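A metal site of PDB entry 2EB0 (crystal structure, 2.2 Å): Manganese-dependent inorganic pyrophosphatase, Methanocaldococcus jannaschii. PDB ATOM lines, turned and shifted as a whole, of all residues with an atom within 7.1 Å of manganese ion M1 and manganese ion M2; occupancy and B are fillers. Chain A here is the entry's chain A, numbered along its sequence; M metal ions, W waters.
The backbone NH (N) of Ala 110 lies within hydrogen-bond range of the side-chain carboxylate (OD2) of Asp 13 (3.0 Å). OD1 of Asp 11 is in hydrogen-bond range of OG of Ser 14 (3.0 Å). The backbone NH of His 7 lies close to the side-chain hydroxyl of Ser 14 (3.4 Å). The backbone carbonyl oxygen (O) of His 88 lies within hydrogen-bond range of the side-chain amino group (NZ) of Lys 294 (2.6 Å). The side-chain carboxylate (OD1) of Asp 11 sits close to a ring nitrogen (NE2) of His 7. A ring nitrogen (ND1) of His 7 sits close to the backbone carbonyl oxygen (O) of Asn 9, 3.4 Å away. The backbone NH (N) of Thr 109 sits close to the side-chain carboxylate (OD2) of Asp 13 (3.4 Å). The backbone NH of Asp 66 lies close to the side-chain hydroxyl of Thr 109, at 3.4 Å.
N of Thr 109 touches manganese ion M1 (3.97 Å).
Merely in contact with manganese ion M2: Lys 204 (3.5 Å) and Ser 14 (3.8 Å). Five residues have an atom within 4 Å of manganese ion M2: His 7, Asp 11, Ser 14, Asp 66 and Lys 204. The nearest printed residue that does not touch manganese ion M2 is Asp 147 (4.5 Å).
Manganese ion M1 is bound by OD1 of Asp 13 (2.2 Å), water W1 (2.3 Å), OD2 of Asp 147 (2.3 Å), OD2 of Asp 66 (2.4 Å) and NE2 of His 88 (2.5 Å).
Manganese ion M2 is bound by OD1 of Asp 66 (2.3 Å). Manganese ion M2 is bound by water W1, 2.3 Å away. Manganese ion M2 is bound by NE2 of His 7. Manganese ion M2 has three donor atoms within binding distance. Slightly farther from manganese ion M2 lies OD2 of Asp 11 (2.7 Å). Slightly farther from manganese ion M2 lies the side-chain carboxylate (OD1) of Asp 11 (2.8 Å).
Water W1 lies within hydrogen-bond range of the side-chain carboxylate of Asp 147 (2.8 Å) and the side-chain carboxylate of Asp 11 (3.0 Å).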
ATOM      1  N   HIS A   7      -8.735  -3.150   5.501  1.00  0.00           N
ATOM      2  CA  HIS A   7      -9.526  -3.862   4.485  1.00  0.00           C
ATOM      3  C   HIS A   7     -10.421  -2.928   3.661  1.00  0.00           C
ATOM      4  O   HIS A   7     -10.573  -1.747   3.987  1.00  0.00           O
ATOM      5  CB  HIS A   7     -10.383  -4.952   5.166  1.00  0.00           C
ATOM      6  CG  HIS A   7     -11.254  -4.442   6.266  1.00  0.00           C
ATOM      7  ND1 HIS A   7     -12.345  -3.621   6.035  1.00  0.00           N
ATOM      8  CD2 HIS A   7     -11.182  -4.605   7.605  1.00  0.00           C
ATOM      9  CE1 HIS A   7     -12.888  -3.291   7.192  1.00  0.00           C
ATOM     10  NE2 HIS A   7     -12.202  -3.874   8.159  1.00  0.00           N
ATOM     11  N   LYS A   8     -10.993  -3.463   2.589  1.00  0.00           N
ATOM     12  CA  LYS A   8     -11.902  -2.672   1.744  1.00  0.00           C
ATOM     13  C   LYS A   8     -13.060  -2.300   2.652  1.00  0.00           C
ATOM     14  O   LYS A   8     -13.282  -2.962   3.678  1.00  0.00           O
ATOM     15  CB  LYS A   8     -12.426  -3.486   0.568  1.00  0.00           C
ATOM     16  CG  LYS A   8     -11.376  -4.051  -0.369  1.00  0.00           C
ATOM     17  CD  LYS A   8     -12.042  -4.478  -1.672  1.00  0.00           C
ATOM     18  CE  LYS A   8     -11.177  -5.434  -2.482  1.00  0.00           C
ATOM     19  NZ  LYS A   8     -11.166  -6.799  -1.861  1.00  0.00           N
ATOM     20  N   ASN A   9     -13.812  -1.273   2.271  1.00  0.00           N
ATOM     21  CA  ASN A   9     -14.932  -0.800   3.100  1.00  0.00           C
ATOM     22  C   ASN A   9     -14.369  -0.717   4.520  1.00  0.00           C
ATOM     23  O   ASN A   9     -14.855  -1.360   5.457  1.00  0.00           O
ATOM     24  CB  ASN A   9     -16.116  -1.767   3.021  1.00  0.00           C
ATOM     25  CG  ASN A   9     -16.661  -1.913   1.604  1.00  0.00           C
ATOM     26  OD1 ASN A   9     -16.685  -0.949   0.831  1.00  0.00           O
ATOM     27  ND2 ASN A   9     -17.097  -3.114   1.243  1.00  0.00           N
ATOM     28  N   PRO A  10     -13.307   0.078   4.689  1.00  0.00           N
ATOM     29  CA  PRO A  10     -12.668   0.244   5.982  1.00  0.00           C
ATOM     30  C   PRO A  10     -13.572   0.784   7.068  1.00  0.00           C
ATOM     31  O   PRO A  10     -14.458   1.597   6.836  1.00  0.00           O
ATOM     32  CB  PRO A  10     -11.500   1.188   5.674  1.00  0.00           C
ATOM     33  CG  PRO A  10     -12.035   2.040   4.549  1.00  0.00           C
ATOM     34  CD  PRO A  10     -12.745   1.009   3.689  1.00  0.00           C
ATOM     35  N   ASP A  11     -13.349   0.281   8.272  1.00  0.00           N
ATOM     36  CA  ASP A  11     -14.087   0.705   9.442  1.00  0.00           C
ATOM     37  C   ASP A  11     -13.067   1.508  10.263  1.00  0.00           C
ATOM     38  O   ASP A  11     -11.937   1.721   9.801  1.00  0.00           O
ATOM     39  CB  ASP A  11     -14.546  -0.526  10.222  1.00  0.00           C
ATOM     40  CG  ASP A  11     -13.400  -1.395  10.690  1.00  0.00           C
ATOM     41  OD1 ASP A  11     -12.349  -1.430  10.001  1.00  0.00           O
ATOM     42  OD2 ASP A  11     -13.552  -2.052  11.732  1.00  0.00           O
ATOM     43  N   THR A  12     -13.444   1.932  11.446  1.00  0.00           N
ATOM     44  CA  THR A  12     -12.545   2.729  12.261  1.00  0.00           C
ATOM     45  C   THR A  12     -11.242   2.017  12.607  1.00  0.00           C
ATOM     46  O   THR A  12     -10.177   2.620  12.550  1.00  0.00           O
ATOM     47  CB  THR A  12     -13.263   3.226  13.527  1.00  0.00           C
ATOM     48  OG1 THR A  12     -14.314   4.110  13.138  1.00  0.00           O
ATOM     49  CG2 THR A  12     -12.302   3.976  14.434  1.00  0.00           C
ATOM     50  N   ASP A  13     -11.305   0.728  12.959  1.00  0.00           N
ATOM     51  CA  ASP A  13     -10.102   0.006  13.313  1.00  0.00           C
ATOM     52  C   ASP A  13      -9.085   0.034  12.167  1.00  0.00           C
ATOM     53  O   ASP A  13      -7.900   0.268  12.385  1.00  0.00           O
ATOM     54  CB  ASP A  13     -10.407  -1.444  13.673  1.00  0.00           C
ATOM     55  CG  ASP A  13      -9.282  -2.099  14.458  1.00  0.00           C
ATOM     56  OD1 ASP A  13      -9.227  -3.342  14.542  1.00  0.00           O
ATOM     57  OD2 ASP A  13      -8.450  -1.356  15.017  1.00  0.00           O
ATOM     58  N   SER A  14      -9.569  -0.215  10.950  1.00  0.00           N
ATOM     59  CA  SER A  14      -8.709  -0.237   9.770  1.00  0.00           C
ATOM     60  C   SER A  14      -8.051   1.119   9.481  1.00  0.00           C
ATOM     61  O   SER A  14      -6.891   1.170   9.076  1.00  0.00           O
ATOM     62  CB  SER A  14      -9.508  -0.668   8.541  1.00  0.00           C
ATOM     63  OG  SER A  14      -9.792  -2.054   8.580  1.00  0.00           O
ATOM     64  N   SER A  17      -5.763   2.064  12.839  1.00  0.00           N
ATOM     65  CA  SER A  17      -4.587   1.201  12.915  1.00  0.00           C
ATOM     66  C   SER A  17      -3.599   1.536  11.814  1.00  0.00           C
ATOM     67  O   SER A  17      -2.401   1.508  12.042  1.00  0.00           O
ATOM     68  CB  SER A  17      -4.969  -0.276  12.826  1.00  0.00           C
ATOM     69  OG  SER A  17      -5.585  -0.718  14.017  1.00  0.00           O
ATOM     70  N   VAL A  65      -3.264  -4.277   7.998  1.00  0.00           N
ATOM     71  CA  VAL A  65      -3.786  -4.270   9.348  1.00  0.00           C
ATOM     72  C   VAL A  65      -5.258  -4.634   9.301  1.00  0.00           C
ATOM     73  O   VAL A  65      -5.961  -4.362   8.328  1.00  0.00           O
ATOM     74  CB  VAL A  65      -3.671  -2.877  10.041  1.00  0.00           C
ATOM     75  CG1 VAL A  65      -2.201  -2.575  10.317  1.00  0.00           C
ATOM     76  CG2 VAL A  65      -4.314  -1.779   9.181  1.00  0.00           C
ATOM     77  N   ASP A  66      -5.695  -5.323  10.347  1.00  0.00           N
ATOM     78  CA  ASP A  66      -7.083  -5.661  10.489  1.00  0.00           C
ATOM     79  C   ASP A  66      -7.729  -6.662   9.514  1.00  0.00           C
ATOM     80  O   ASP A  66      -8.947  -6.670   9.351  1.00  0.00           O
ATOM     81  CB  ASP A  66      -7.876  -4.364  10.461  1.00  0.00           C
ATOM     82  CG  ASP A  66      -9.242  -4.504  11.033  1.00  0.00           C
ATOM     83  OD1 ASP A  66     -10.072  -3.645  10.738  1.00  0.00           O
ATOM     84  OD2 ASP A  66      -9.472  -5.480  11.776  1.00  0.00           O
ATOM     85  N   HIS A  67      -6.921  -7.485   8.850  1.00  0.00           N
ATOM     86  CA  HIS A  67      -7.493  -8.482   7.954  1.00  0.00           C
ATOM     87  C   HIS A  67      -6.454  -9.420   7.367  1.00  0.00           C
ATOM     88  O   HIS A  67      -5.268  -9.083   7.296  1.00  0.00           O
ATOM     89  CB  HIS A  67      -8.308  -7.827   6.820  1.00  0.00           C
ATOM     90  CG  HIS A  67      -7.495  -7.173   5.745  1.00  0.00           C
ATOM     91  ND1 HIS A  67      -6.735  -6.042   5.960  1.00  0.00           N
ATOM     92  CD2 HIS A  67      -7.318  -7.493   4.440  1.00  0.00           C
ATOM     93  CE1 HIS A  67      -6.142  -5.685   4.836  1.00  0.00           C
ATOM     94  NE2 HIS A  67      -6.484  -6.555   3.888  1.00  0.00           N
ATOM     95  N   ASP A  87      -3.051  -8.078  12.969  1.00  0.00           N
ATOM     96  CA  ASP A  87      -4.486  -8.305  12.923  1.00  0.00           C
ATOM     97  C   ASP A  87      -5.001  -9.050  14.147  1.00  0.00           C
ATOM     98  O   ASP A  87      -4.233  -9.374  15.063  1.00  0.00           O
ATOM     99  CB  ASP A  87      -4.737  -9.131  11.652  1.00  0.00           C
ATOM    100  CG  ASP A  87      -6.188  -9.368  11.380  1.00  0.00           C
ATOM    101  OD1 ASP A  87      -6.493 -10.399  10.749  1.00  0.00           O
ATOM    102  OD2 ASP A  87      -7.022  -8.525  11.775  1.00  0.00           O
ATOM    103  N   HIS A  88      -6.307  -9.309  14.173  1.00  0.00           N
ATOM    104  CA  HIS A  88      -6.927 -10.021  15.279  1.00  0.00           C
ATOM    105  C   HIS A  88      -7.940 -11.050  14.773  1.00  0.00           C
ATOM    106  O   HIS A  88      -8.736 -11.578  15.542  1.00  0.00           O
ATOM    107  CB  HIS A  88      -7.574  -9.052  16.262  1.00  0.00           C
ATOM    108  CG  HIS A  88      -8.719  -8.279  15.689  1.00  0.00           C
ATOM    109  ND1 HIS A  88     -10.008  -8.387  16.182  1.00  0.00           N
ATOM    110  CD2 HIS A  88      -8.776  -7.382  14.681  1.00  0.00           C
ATOM    111  CE1 HIS A  88     -10.806  -7.599  15.494  1.00  0.00           C
ATOM    112  NE2 HIS A  88     -10.089  -6.980  14.571  1.00  0.00           N
ATOM    113  N   HIS A  89      -7.903 -11.322  13.464  1.00  0.00           N
ATOM    114  CA  HIS A  89      -8.795 -12.297  12.863  1.00  0.00           C
ATOM    115  C   HIS A  89      -8.051 -13.625  12.716  1.00  0.00           C
ATOM    116  O   HIS A  89      -6.868 -13.726  13.028  1.00  0.00           O
ATOM    117  CB  HIS A  89      -9.244 -11.827  11.475  1.00  0.00           C
ATOM    118  CG  HIS A  89     -10.099 -10.598  11.483  1.00  0.00           C
ATOM    119  ND1 HIS A  89      -9.578  -9.338  11.654  1.00  0.00           N
ATOM    120  CD2 HIS A  89     -11.446 -10.445  11.362  1.00  0.00           C
ATOM    121  CE1 HIS A  89     -10.572  -8.458  11.639  1.00  0.00           C
ATOM    122  NE2 HIS A  89     -11.704  -9.105  11.470  1.00  0.00           N
ATOM    123  N   GLY A 107     -10.189  -8.002  20.882  1.00  0.00           N
ATOM    124  CA  GLY A 107     -11.276  -7.225  20.289  1.00  0.00           C
ATOM    125  C   GLY A 107     -11.003  -6.363  19.068  1.00  0.00           C
ATOM    126  O   GLY A 107     -11.911  -6.140  18.266  1.00  0.00           O
ATOM    127  N   SER A 108      -9.789  -5.852  18.913  1.00  0.00           N
ATOM    128  CA  SER A 108      -9.508  -5.020  17.753  1.00  0.00           C
ATOM    129  C   SER A 108      -8.035  -5.021  17.420  1.00  0.00           C
ATOM    130  O   SER A 108      -7.212  -5.520  18.187  1.00  0.00           O
ATOM    131  CB  SER A 108      -9.940  -3.572  18.026  1.00  0.00           C
ATOM    132  OG  SER A 108      -9.057  -2.949  18.941  1.00  0.00           O
ATOM    133  N   THR A 109      -7.704  -4.450  16.260  1.00  0.00           N
ATOM    134  CA  THR A 109      -6.308  -4.367  15.861  1.00  0.00           C
ATOM    135  C   THR A 109      -5.663  -3.259  16.696  1.00  0.00           C
ATOM    136  O   THR A 109      -4.481  -3.351  17.036  1.00  0.00           O
ATOM    137  CB  THR A 109      -6.183  -4.049  14.338  1.00  0.00           C
ATOM    138  OG1 THR A 109      -6.759  -5.109  13.573  1.00  0.00           O
ATOM    139  CG2 THR A 109      -4.706  -3.902  13.934  1.00  0.00           C
ATOM    140  N   ALA A 110      -6.435  -2.238  17.050  1.00  0.00           N
ATOM    141  CA  ALA A 110      -5.925  -1.143  17.867  1.00  0.00           C
ATOM    142  C   ALA A 110      -5.463  -1.664  19.224  1.00  0.00           C
ATOM    143  O   ALA A 110      -4.447  -1.219  19.769  1.00  0.00           O
ATOM    144  CB  ALA A 110      -7.003  -0.060  18.051  1.00  0.00           C
ATOM    145  N   ALA A 143     -11.097   3.090  17.993  1.00  0.00           N
ATOM    146  CA  ALA A 143     -11.068   1.829  17.260  1.00  0.00           C
ATOM    147  C   ALA A 143     -11.523   0.692  18.173  1.00  0.00           C
ATOM    148  O   ALA A 143     -12.327  -0.150  17.783  1.00  0.00           O
ATOM    149  CB  ALA A 143      -9.657   1.570  16.753  1.00  0.00           C
ATOM    150  N   ASP A 147     -14.837  -1.277  17.417  1.00  0.00           N
ATOM    151  CA  ASP A 147     -14.720  -2.720  17.208  1.00  0.00           C
ATOM    152  C   ASP A 147     -15.422  -3.609  18.227  1.00  0.00           C
ATOM    153  O   ASP A 147     -15.903  -4.696  17.892  1.00  0.00           O
ATOM    154  CB  ASP A 147     -13.247  -3.104  17.134  1.00  0.00           C
ATOM    155  CG  ASP A 147     -12.827  -3.568  15.775  1.00  0.00           C
ATOM    156  OD1 ASP A 147     -13.456  -3.118  14.779  1.00  0.00           O
ATOM    157  OD2 ASP A 147     -11.874  -4.365  15.697  1.00  0.00           O
ATOM    158  N   ASP A 202     -20.317  -1.347   4.979  1.00  0.00           N
ATOM    159  CA  ASP A 202     -19.541  -2.341   5.713  1.00  0.00           C
ATOM    160  C   ASP A 202     -19.799  -3.771   5.246  1.00  0.00           C
ATOM    161  O   ASP A 202     -20.346  -4.589   5.986  1.00  0.00           O
ATOM    162  CB  ASP A 202     -19.846  -2.228   7.208  1.00  0.00           C
ATOM    163  CG  ASP A 202     -19.215  -3.336   8.021  1.00  0.00           C
ATOM    164  OD1 ASP A 202     -18.014  -3.603   7.851  1.00  0.00           O
ATOM    165  OD2 ASP A 202     -19.933  -3.947   8.839  1.00  0.00           O
ATOM    166  N   LYS A 204     -18.219  -7.402   3.749  1.00  0.00           N
ATOM    167  CA  LYS A 204     -16.988  -8.185   3.673  1.00  0.00           C
ATOM    168  C   LYS A 204     -17.188  -9.450   2.841  1.00  0.00           C
ATOM    169  O   LYS A 204     -18.258 -10.050   2.869  1.00  0.00           O
ATOM    170  CB  LYS A 204     -16.484  -8.546   5.075  1.00  0.00           C
ATOM    171  CG  LYS A 204     -15.772  -7.400   5.773  1.00  0.00           C
ATOM    172  CD  LYS A 204     -15.160  -7.800   7.108  1.00  0.00           C
ATOM    173  CE  LYS A 204     -14.291  -6.667   7.647  1.00  0.00           C
ATOM    174  NZ  LYS A 204     -13.730  -6.930   9.018  1.00  0.00           N
ATOM    175  N   ARG A 293     -19.629 -10.345  13.433  1.00  0.00           N
ATOM    176  CA  ARG A 293     -19.624 -11.134  12.209  1.00  0.00           C
ATOM    177  C   ARG A 293     -18.530 -12.189  12.274  1.00  0.00           C
ATOM    178  O   ARG A 293     -18.793 -13.382  12.123  1.00  0.00           O
ATOM    179  CB  ARG A 293     -19.385 -10.225  10.995  1.00  0.00           C
ATOM    180  CG  ARG A 293     -19.068 -10.943   9.691  1.00  0.00           C
ATOM    181  CD  ARG A 293     -18.977  -9.943   8.558  1.00  0.00           C
ATOM    182  NE  ARG A 293     -18.233  -8.756   8.972  1.00  0.00           N
ATOM    183  CZ  ARG A 293     -18.421  -7.544   8.460  1.00  0.00           C
ATOM    184  NH1 ARG A 293     -19.328  -7.349   7.509  1.00  0.00           N
ATOM    185  NH2 ARG A 293     -17.709  -6.521   8.904  1.00  0.00           N
ATOM    186  N   LYS A 294     -17.307 -11.743  12.540  1.00  0.00           N
ATOM    187  CA  LYS A 294     -16.162 -12.628  12.616  1.00  0.00           C
ATOM    188  C   LYS A 294     -16.302 -13.758  13.626  1.00  0.00           C
ATOM    189  O   LYS A 294     -15.980 -14.914  13.337  1.00  0.00           O
ATOM    190  CB  LYS A 294     -14.897 -11.835  12.969  1.00  0.00           C
ATOM    191  CG  LYS A 294     -14.933 -11.199  14.350  1.00  0.00           C
ATOM    192  CD  LYS A 294     -13.595 -10.623  14.714  1.00  0.00           C
ATOM    193  CE  LYS A 294     -12.540 -11.711  14.813  1.00  0.00           C
ATOM    194  NZ  LYS A 294     -11.235 -11.155  15.228  1.00  0.00           N
HETATM  195 MN    MN M   1     -10.739  -4.727  13.716  1.00  0.00          MN
HETATM  196 MN    MN M   2     -12.278  -4.139  10.515  1.00  0.00          MN
HETATM  197  O   HOH W   1     -12.727  -4.824  12.648  1.00  0.00           O
